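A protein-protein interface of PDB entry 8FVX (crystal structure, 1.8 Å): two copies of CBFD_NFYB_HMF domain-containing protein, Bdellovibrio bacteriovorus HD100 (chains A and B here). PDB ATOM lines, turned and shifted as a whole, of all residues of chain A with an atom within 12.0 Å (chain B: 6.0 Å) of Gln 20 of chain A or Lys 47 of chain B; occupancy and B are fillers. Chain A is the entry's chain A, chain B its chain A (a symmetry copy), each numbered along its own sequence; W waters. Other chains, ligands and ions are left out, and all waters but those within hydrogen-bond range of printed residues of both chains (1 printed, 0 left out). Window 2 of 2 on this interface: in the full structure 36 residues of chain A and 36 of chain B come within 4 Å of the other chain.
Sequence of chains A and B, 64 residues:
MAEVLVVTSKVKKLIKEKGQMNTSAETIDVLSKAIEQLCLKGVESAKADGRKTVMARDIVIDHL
O of Arg 51 of chain B lies close to SD of Met 21 of chain A (3.4 Å).
The side-chain amide oxygen of Gln 20 of chain A lies within hydrogen-bond range of the side-chain amino group of Lys 47 of chain B, at 2.6 Å.
The backbone carbonyl oxygen (O) of Lys 52 of chain B lies within hydrogen-bond range of the backbone NH (N) of Asn 22 of chain A, at 2.9 Å.
The side-chain amino group (NZ) of Lys 52 of chain B lies within hydrogen-bond range of the backbone carbonyl oxygen (O) of Gln 20 of chain A (2.8 Å).
Of the 16 printed residues of chain A, 4 touch a printed residue of chain B.
Hydrophobic or aromatic side chains of chain A within 4 Å of the printed part of chain B: Met 21.
Of the 11 printed residues of chain B, 4 touch a printed residue of chain A.
Printed residues of chain B that touch a printed residue of chain A: Val 43, Lys 47, Arg 51 and Lys 52.
Hydrophobic or aromatic side chains of chain B that line the printed part of chain A: Val 43.
Among the printed residues, 8 pairs touch across the chains.
CA of Gly 19 of chain A touches CG1 of Val 43 of chain B (3.6 Å).
O of Gly 19 of chain A touches CD of Lys 47 of chain B (3.8 Å).
CE of Met 21 of chain A touches CG of Lys 47 of chain B, 3.3 Å away.
Met 21 of chain A touches Lys 52 of chain B.
Printed residues of chain B within 4 Å of Gln 20 of chain A: Lys 47 (2.6 Å) and Lys 52 (2.8 Å).
Of chain A, only Gly 19, Gln 20 and Met 21 come within 4 Å of Lys 47 of chain B.
No residue of chain A comes within 4 Å of Glu 44 of chain B.
No residue of chain A comes within 4 Å of Ala 46 of chain B.
No residue of chain A comes within 4 Å of Ala 48 of chain B.
No residue of chain A comes within 4 Å of Asp 49 of chain B.
No residue of chain A comes within 4 Å of Gly 50 of chain B.
Of chain A, only Met 21 (3.4 Å) comes within 4 Å of Arg 51 of chain B.
Of chain A, only Gln 20 (2.8 Å), Met 21 (3.4 Å) and Asn 22 (2.9 Å) come within 4 Å of Lys 52 of chain B.
Printed residues of chain B within 4 Å of Gly 19 of chain A: Val 43 and Lys 47.
Printed residues of chain B within 4 Å of Met 21 of chain A: Lys 47 (3.3 Å), Arg 51 (3.4 Å) and Lys 52 (3.4 Å).
Printed residues of chain B within 4 Å of Asn 22 of chain A: Lys 52 (2.9 Å).
Ile 15 of chain A touches none of the printed residues of chain B.
Lys 18 of chain A touches none of the printed residues of chain B.
The nearest residue of chain B that does not touch Gln 20 of chain A is Val 43 of chain B (5.5 Å).
O of Ile 15 of chain A is in hydrogen-bond range of N of Gln 20 of chain A (3.3 Å).
The backbone carbonyl oxygen of Lys 18 of chain A sits at hydrogen-bond distance from the side-chain amide nitrogen of Gln 20 of chain A (3.4 Å).
O of Met 21 of chain A sits close to N of Lys 16 of chain A, at 3.4 Å.
N of Met 21 of chain A lies within hydrogen-bond range of O of Ile 15 of chain A, 3.4 Å away.
OD2 of Asp 49 of chain B is in salt-bridge range of NE of Arg 51 of chain B (2.8 Å).
The side-chain amino group (NZ) of Lys 16 of chain A is in hydrogen-bond range of the side-chain amide oxygen (OD1) of Asn 22 of chain A, 3.1 Å away.
No position is printed for both chains.
Of the 8 pairs that touch across the chains among the printed residues, none has its exchanged pair printed and touching as well.
Water W1 bridges OE1 of Gln 20 of chain A (2.5 Å) and NZ of Lys 47 of chain B (3.1 Å).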
ATOM      1  N   LYS A  10      16.018 -31.800  40.718  1.00  0.00           N
ATOM      2  CA  LYS A  10      17.239 -31.527  39.966  1.00  0.00           C
ATOM      3  C   LYS A  10      17.019 -31.616  38.457  1.00  0.00           C
ATOM      4  O   LYS A  10      17.728 -30.949  37.694  1.00  0.00           O
ATOM      5  CB  LYS A  10      18.346 -32.482  40.417  1.00  0.00           C
ATOM      6  CG  LYS A  10      18.650 -32.380  41.914  1.00  0.00           C
ATOM      7  CD  LYS A  10      19.977 -33.053  42.289  1.00  0.00           C
ATOM      8  CE  LYS A  10      20.300 -32.796  43.766  1.00  0.00           C
ATOM      9  NZ  LYS A  10      21.476 -33.563  44.251  1.00  0.00           N
ATOM     10  N   VAL A  11      16.059 -32.436  38.020  1.00  0.00           N
ATOM     11  CA  VAL A  11      15.667 -32.467  36.614  1.00  0.00           C
ATOM     12  C   VAL A  11      15.012 -31.148  36.215  1.00  0.00           C
ATOM     13  O   VAL A  11      15.384 -30.536  35.204  1.00  0.00           O
ATOM     14  CB  VAL A  11      14.731 -33.658  36.344  1.00  0.00           C
ATOM     15  CG1 VAL A  11      13.989 -33.459  35.035  1.00  0.00           C
ATOM     16  CG2 VAL A  11      15.516 -34.975  36.356  1.00  0.00           C
ATOM     17  N   LYS A  12      14.019 -30.698  36.996  1.00  0.00           N
ATOM     18  CA  LYS A  12      13.403 -29.394  36.736  1.00  0.00           C
ATOM     19  C   LYS A  12      14.434 -28.276  36.733  1.00  0.00           C
ATOM     20  O   LYS A  12      14.339 -27.342  35.930  1.00  0.00           O
ATOM     21  CB  LYS A  12      12.318 -29.094  37.766  1.00  0.00           C
ATOM     22  CG  LYS A  12      11.288 -30.158  37.943  1.00  0.00           C
ATOM     23  CD  LYS A  12       9.908 -29.551  38.076  1.00  0.00           C
ATOM     24  CE  LYS A  12       8.846 -30.608  38.281  1.00  0.00           C
ATOM     25  NZ  LYS A  12       7.539 -30.210  37.662  1.00  0.00           N
ATOM     26  N   LYS A  13      15.418 -28.344  37.636  1.00  0.00           N
ATOM     27  CA  LYS A  13      16.430 -27.297  37.713  1.00  0.00           C
ATOM     28  C   LYS A  13      17.309 -27.291  36.469  1.00  0.00           C
ATOM     29  O   LYS A  13      17.655 -26.223  35.953  1.00  0.00           O
ATOM     30  CB  LYS A  13      17.289 -27.478  38.967  1.00  0.00           C
ATOM     31  CG  LYS A  13      18.585 -26.677  38.915  1.00  0.00           C
ATOM     32  CD  LYS A  13      19.376 -26.751  40.212  1.00  0.00           C
ATOM     33  CE  LYS A  13      20.770 -26.182  40.004  1.00  0.00           C
ATOM     34  NZ  LYS A  13      21.784 -26.758  40.928  1.00  0.00           N
ATOM     35  N   LEU A  14      17.687 -28.475  35.979  1.00  0.00           N
ATOM     36  CA  LEU A  14      18.496 -28.562  34.770  1.00  0.00           C
ATOM     37  C   LEU A  14      17.747 -27.990  33.578  1.00  0.00           C
ATOM     38  O   LEU A  14      18.297 -27.206  32.792  1.00  0.00           O
ATOM     39  CB  LEU A  14      18.874 -30.024  34.495  1.00  0.00           C
ATOM     40  CG  LEU A  14      19.553 -30.278  33.139  1.00  0.00           C
ATOM     41  CD1 LEU A  14      20.930 -29.596  33.059  1.00  0.00           C
ATOM     42  CD2 LEU A  14      19.689 -31.766  32.859  1.00  0.00           C
ATOM     43  N   ILE A  15      16.485 -28.388  33.427  1.00  0.00           N
ATOM     44  CA  ILE A  15      15.710 -27.996  32.258  1.00  0.00           C
ATOM     45  C   ILE A  15      15.441 -26.500  32.274  1.00  0.00           C
ATOM     46  O   ILE A  15      15.468 -25.843  31.227  1.00  0.00           O
ATOM     47  CB  ILE A  15      14.416 -28.820  32.203  1.00  0.00           C
ATOM     48  CG1 ILE A  15      14.751 -30.246  31.777  1.00  0.00           C
ATOM     49  CG2 ILE A  15      13.398 -28.169  31.270  1.00  0.00           C
ATOM     50  CD1 ILE A  15      13.606 -31.228  31.974  1.00  0.00           C
ATOM     51  N   LYS A  16      15.205 -25.935  33.461  1.00  0.00           N
ATOM     52  CA  LYS A  16      14.991 -24.491  33.568  1.00  0.00           C
ATOM     53  C   LYS A  16      16.285 -23.714  33.361  1.00  0.00           C
ATOM     54  O   LYS A  16      16.319 -22.712  32.633  1.00  0.00           O
ATOM     55  CB  LYS A  16      14.386 -24.145  34.930  1.00  0.00           C
ATOM     56  CG  LYS A  16      14.071 -22.667  35.074  1.00  0.00           C
ATOM     57  CD  LYS A  16      13.174 -22.143  33.958  1.00  0.00           C
ATOM     58  CE  LYS A  16      11.741 -22.622  34.120  1.00  0.00           C
ATOM     59  NZ  LYS A  16      11.326 -22.770  35.549  1.00  0.00           N
ATOM     60  N   GLU A  17      17.365 -24.147  34.009  1.00  0.00           N
ATOM     61  CA  GLU A  17      18.577 -23.337  34.011  1.00  0.00           C
ATOM     62  C   GLU A  17      19.307 -23.427  32.674  1.00  0.00           C
ATOM     63  O   GLU A  17      19.842 -22.427  32.183  1.00  0.00           O
ATOM     64  CB  GLU A  17      19.456 -23.768  35.188  1.00  0.00           C
ATOM     65  CG  GLU A  17      18.942 -23.142  36.498  1.00  0.00           C
ATOM     66  CD  GLU A  17      19.898 -23.235  37.672  1.00  0.00           C
ATOM     67  OE1 GLU A  17      19.478 -22.869  38.801  1.00  0.00           O
ATOM     68  OE2 GLU A  17      21.037 -23.708  37.480  1.00  0.00           O
ATOM     69  N   LYS A  18      19.295 -24.595  32.036  1.00  0.00           N
ATOM     70  CA  LYS A  18      20.040 -24.770  30.798  1.00  0.00           C
ATOM     71  C   LYS A  18      19.183 -24.565  29.556  1.00  0.00           C
ATOM     72  O   LYS A  18      19.729 -24.280  28.481  1.00  0.00           O
ATOM     73  CB  LYS A  18      20.688 -26.164  30.772  1.00  0.00           C
ATOM     74  CG  LYS A  18      21.932 -26.267  29.893  1.00  0.00           C
ATOM     75  CD  LYS A  18      23.125 -26.829  30.658  1.00  0.00           C
ATOM     76  CE  LYS A  18      23.772 -25.774  31.553  1.00  0.00           C
ATOM     77  NZ  LYS A  18      25.111 -26.218  32.061  1.00  0.00           N
ATOM     78  N   GLY A  19      17.863 -24.639  29.681  1.00  0.00           N
ATOM     79  CA  GLY A  19      17.021 -24.583  28.509  1.00  0.00           C
ATOM     80  C   GLY A  19      15.900 -23.575  28.546  1.00  0.00           C
ATOM     81  O   GLY A  19      15.200 -23.408  27.544  1.00  0.00           O
ATOM     82  N   GLN A  20      15.721 -22.893  29.685  1.00  0.00           N
ATOM     83  CA  GLN A  20      14.702 -21.869  29.896  1.00  0.00           C
ATOM     84  C   GLN A  20      13.269 -22.432  29.920  1.00  0.00           C
ATOM     85  O   GLN A  20      12.298 -21.670  29.865  1.00  0.00           O
ATOM     86  CB  GLN A  20      14.839 -20.731  28.858  1.00  0.00           C
ATOM     87  CG  GLN A  20      16.318 -20.262  28.569  1.00  0.00           C
ATOM     88  CD  GLN A  20      16.971 -20.900  27.330  1.00  0.00           C
ATOM     89  OE1 GLN A  20      16.411 -20.886  26.232  1.00  0.00           O
ATOM     90  NE2 GLN A  20      18.153 -21.484  27.518  1.00  0.00           N
ATOM     91  N   MET A  21      13.112 -23.751  30.053  1.00  0.00           N
ATOM     92  CA  MET A  21      11.838 -24.468  30.024  1.00  0.00           C
ATOM     93  C   MET A  21      11.340 -24.901  31.406  1.00  0.00           C
ATOM     94  O   MET A  21      12.121 -25.163  32.322  1.00  0.00           O
ATOM     95  CB  MET A  21      11.950 -25.712  29.120  1.00  0.00           C
ATOM     96  CG  MET A  21      12.647 -25.492  27.786  1.00  0.00           C
ATOM     97  SD  MET A  21      11.365 -24.797  26.691  1.00  0.00           S
ATOM     98  CE  MET A  21      12.152 -23.251  26.262  1.00  0.00           C
ATOM     99  N   ASN A  22      10.011 -24.974  31.535  1.00  0.00           N
ATOM    100  CA  ASN A  22       9.361 -25.720  32.602  1.00  0.00           C
ATOM    101  C   ASN A  22       9.357 -27.211  32.267  1.00  0.00           C
ATOM    102  O   ASN A  22       9.702 -27.627  31.159  1.00  0.00           O
ATOM    103  CB  ASN A  22       7.921 -25.250  32.814  1.00  0.00           C
ATOM    104  CG  ASN A  22       7.833 -23.800  33.236  1.00  0.00           C
ATOM    105  OD1 ASN A  22       8.632 -23.325  34.040  1.00  0.00           O
ATOM    106  ND2 ASN A  22       6.842 -23.095  32.711  1.00  0.00           N
ATOM    107  N   THR A  23       8.937 -28.024  33.237  1.00  0.00           N
ATOM    108  CA  THR A  23       8.942 -29.478  33.104  1.00  0.00           C
ATOM    109  C   THR A  23       7.584 -30.017  33.520  1.00  0.00           C
ATOM    110  O   THR A  23       7.201 -29.878  34.683  1.00  0.00           O
ATOM    111  CB  THR A  23      10.038 -30.105  33.975  1.00  0.00           C
ATOM    112  OG1 THR A  23      11.310 -29.520  33.670  1.00  0.00           O
ATOM    113  CG2 THR A  23      10.100 -31.627  33.776  1.00  0.00           C
ATOM    114  N   SER A  24       6.874 -30.660  32.591  1.00  0.00           N
ATOM    115  CA  SER A  24       5.557 -31.208  32.910  1.00  0.00           C
ATOM    116  C   SER A  24       5.664 -32.443  33.813  1.00  0.00           C
ATOM    117  O   SER A  24       6.689 -33.131  33.867  1.00  0.00           O
ATOM    118  CB  SER A  24       4.809 -31.577  31.632  1.00  0.00           C
ATOM    119  OG  SER A  24       5.085 -32.921  31.266  1.00  0.00           O
ATOM    120  N   THR A  27       6.529 -35.560  31.930  1.00  0.00           N
ATOM    121  CA  THR A  27       7.946 -35.665  31.592  1.00  0.00           C
ATOM    122  C   THR A  27       8.715 -36.395  32.685  1.00  0.00           C
ATOM    123  O   THR A  27       9.575 -37.239  32.398  1.00  0.00           O
ATOM    124  CB  THR A  27       8.526 -34.271  31.370  1.00  0.00           C
ATOM    125  OG1 THR A  27       7.806 -33.635  30.304  1.00  0.00           O
ATOM    126  CG2 THR A  27      10.006 -34.351  31.017  1.00  0.00           C
ATOM    127  N   GLY B  42      15.134 -33.146  25.244  1.00  0.00           N
ATOM    128  CA  GLY B  42      13.768 -32.686  25.425  1.00  0.00           C
ATOM    129  C   GLY B  42      13.646 -31.181  25.298  1.00  0.00           C
ATOM    130  O   GLY B  42      12.670 -30.678  24.738  1.00  0.00           O
ATOM    131  N   VAL B  43      14.633 -30.441  25.826  1.00  0.00           N
ATOM    132  CA  VAL B  43      14.668 -28.988  25.653  1.00  0.00           C
ATOM    133  C   VAL B  43      14.711 -28.638  24.173  1.00  0.00           C
ATOM    134  O   VAL B  43      13.985 -27.750  23.705  1.00  0.00           O
ATOM    135  CB  VAL B  43      15.868 -28.377  26.406  1.00  0.00           C
ATOM    136  CG1 VAL B  43      16.072 -26.930  25.982  1.00  0.00           C
ATOM    137  CG2 VAL B  43      15.676 -28.468  27.926  1.00  0.00           C
ATOM    138  N   GLU B  44      15.556 -29.345  23.413  1.00  0.00           N
ATOM    139  CA  GLU B  44      15.681 -29.079  21.982  1.00  0.00           C
ATOM    140  C   GLU B  44      14.351 -29.281  21.282  1.00  0.00           C
ATOM    141  O   GLU B  44      13.951 -28.463  20.451  1.00  0.00           O
ATOM    142  CB  GLU B  44      16.732 -30.002  21.365  1.00  0.00           C
ATOM    143  CG  GLU B  44      18.139 -29.743  21.872  1.00  0.00           C
ATOM    144  CD  GLU B  44      18.651 -28.372  21.486  1.00  0.00           C
ATOM    145  OE1 GLU B  44      18.898 -28.151  20.280  1.00  0.00           O
ATOM    146  OE2 GLU B  44      18.814 -27.522  22.394  1.00  0.00           O
ATOM    147  N   SER B  45      13.659 -30.380  21.606  1.00  0.00           N
ATOM    148  CA  SER B  45      12.381 -30.692  20.975  1.00  0.00           C
ATOM    149  C   SER B  45      11.312 -29.667  21.338  1.00  0.00           C
ATOM    150  O   SER B  45      10.588 -29.174  20.460  1.00  0.00           O
ATOM    151  CB  SER B  45      11.936 -32.100  21.387  1.00  0.00           C
ATOM    152  OG  SER B  45      10.621 -32.362  20.928  1.00  0.00           O
ATOM    153  N   ALA B  46      11.206 -29.323  22.625  1.00  0.00           N
ATOM    154  CA  ALA B  46      10.201 -28.356  23.059  1.00  0.00           C
ATOM    155  C   ALA B  46      10.436 -26.994  22.413  1.00  0.00           C
ATOM    156  O   ALA B  46       9.498 -26.366  21.900  1.00  0.00           O
ATOM    157  CB  ALA B  46      10.203 -28.240  24.584  1.00  0.00           C
ATOM    158  N   LYS B  47      11.687 -26.529  22.404  1.00  0.00           N
ATOM    159  CA  LYS B  47      11.961 -25.214  21.826  1.00  0.00           C
ATOM    160  C   LYS B  47      11.702 -25.206  20.324  1.00  0.00           C
ATOM    161  O   LYS B  47      11.184 -24.215  19.779  1.00  0.00           O
ATOM    162  CB  LYS B  47      13.399 -24.801  22.124  1.00  0.00           C
ATOM    163  CG  LYS B  47      13.622 -24.454  23.569  1.00  0.00           C
ATOM    164  CD  LYS B  47      14.921 -23.699  23.755  1.00  0.00           C
ATOM    165  CE  LYS B  47      14.771 -22.248  23.297  1.00  0.00           C
ATOM    166  NZ  LYS B  47      15.962 -21.456  23.695  1.00  0.00           N
ATOM    167  N   ALA B  48      12.040 -26.301  19.639  1.00  0.00           N
ATOM    168  CA  ALA B  48      11.807 -26.370  18.201  1.00  0.00           C
ATOM    169  C   ALA B  48      10.322 -26.262  17.876  1.00  0.00           C
ATOM    170  O   ALA B  48       9.957 -25.825  16.777  1.00  0.00           O
ATOM    171  CB  ALA B  48      12.389 -27.666  17.626  1.00  0.00           C
ATOM    172  N   ASP B  49       9.458 -26.662  18.811  1.00  0.00           N
ATOM    173  CA  ASP B  49       8.017 -26.530  18.647  1.00  0.00           C
ATOM    174  C   ASP B  49       7.505 -25.187  19.136  1.00  0.00           C
ATOM    175  O   ASP B  49       6.294 -24.955  19.098  1.00  0.00           O
ATOM    176  CB  ASP B  49       7.284 -27.667  19.384  1.00  0.00           C
ATOM    177  CG  ASP B  49       5.895 -27.935  18.816  1.00  0.00           C
ATOM    178  OD1 ASP B  49       5.734 -27.887  17.578  1.00  0.00           O
ATOM    179  OD2 ASP B  49       4.958 -28.183  19.606  1.00  0.00           O
ATOM    180  N   GLY B  50       8.397 -24.301  19.581  1.00  0.00           N
ATOM    181  CA  GLY B  50       8.008 -23.001  20.082  1.00  0.00           C
ATOM    182  C   GLY B  50       7.339 -23.014  21.431  1.00  0.00           C
ATOM    183  O   GLY B  50       6.614 -22.067  21.757  1.00  0.00           O
ATOM    184  N   ARG B  51       7.562 -24.050  22.235  1.00  0.00           N
ATOM    185  CA  ARG B  51       6.920 -24.170  23.535  1.00  0.00           C
ATOM    186  C   ARG B  51       7.870 -23.760  24.656  1.00  0.00           C
ATOM    187  O   ARG B  51       9.081 -23.619  24.468  1.00  0.00           O
ATOM    188  CB  ARG B  51       6.416 -25.599  23.753  1.00  0.00           C
ATOM    189  CG  ARG B  51       5.151 -25.910  22.967  1.00  0.00           C
ATOM    190  CD  ARG B  51       4.697 -27.348  23.191  1.00  0.00           C
ATOM    191  NE  ARG B  51       5.425 -28.299  22.351  1.00  0.00           N
ATOM    192  CZ  ARG B  51       6.361 -29.127  22.793  1.00  0.00           C
ATOM    193  NH1 ARG B  51       6.741 -29.129  24.059  1.00  0.00           N
ATOM    194  NH2 ARG B  51       6.913 -29.992  21.948  1.00  0.00           N
ATOM    195  N   LYS B  52       7.296 -23.568  25.844  1.00  0.00           N
ATOM    196  CA  LYS B  52       8.056 -23.162  27.020  1.00  0.00           C
ATOM    197  C   LYS B  52       8.086 -24.247  28.091  1.00  0.00           C
ATOM    198  O   LYS B  52       8.558 -23.988  29.200  1.00  0.00           O
ATOM    199  CB  LYS B  52       7.473 -21.869  27.598  1.00  0.00           C
ATOM    200  CG  LYS B  52       7.711 -20.617  26.742  1.00  0.00           C
ATOM    201  CD  LYS B  52       8.865 -19.752  27.265  1.00  0.00           C
ATOM    202  CE  LYS B  52      10.232 -20.373  26.998  1.00  0.00           C
ATOM    203  NZ  LYS B  52      11.289 -19.878  27.929  1.00  0.00           N
HETATM  204  O   HOH W   1      14.732 -19.194  25.397  1.00  0.00           O
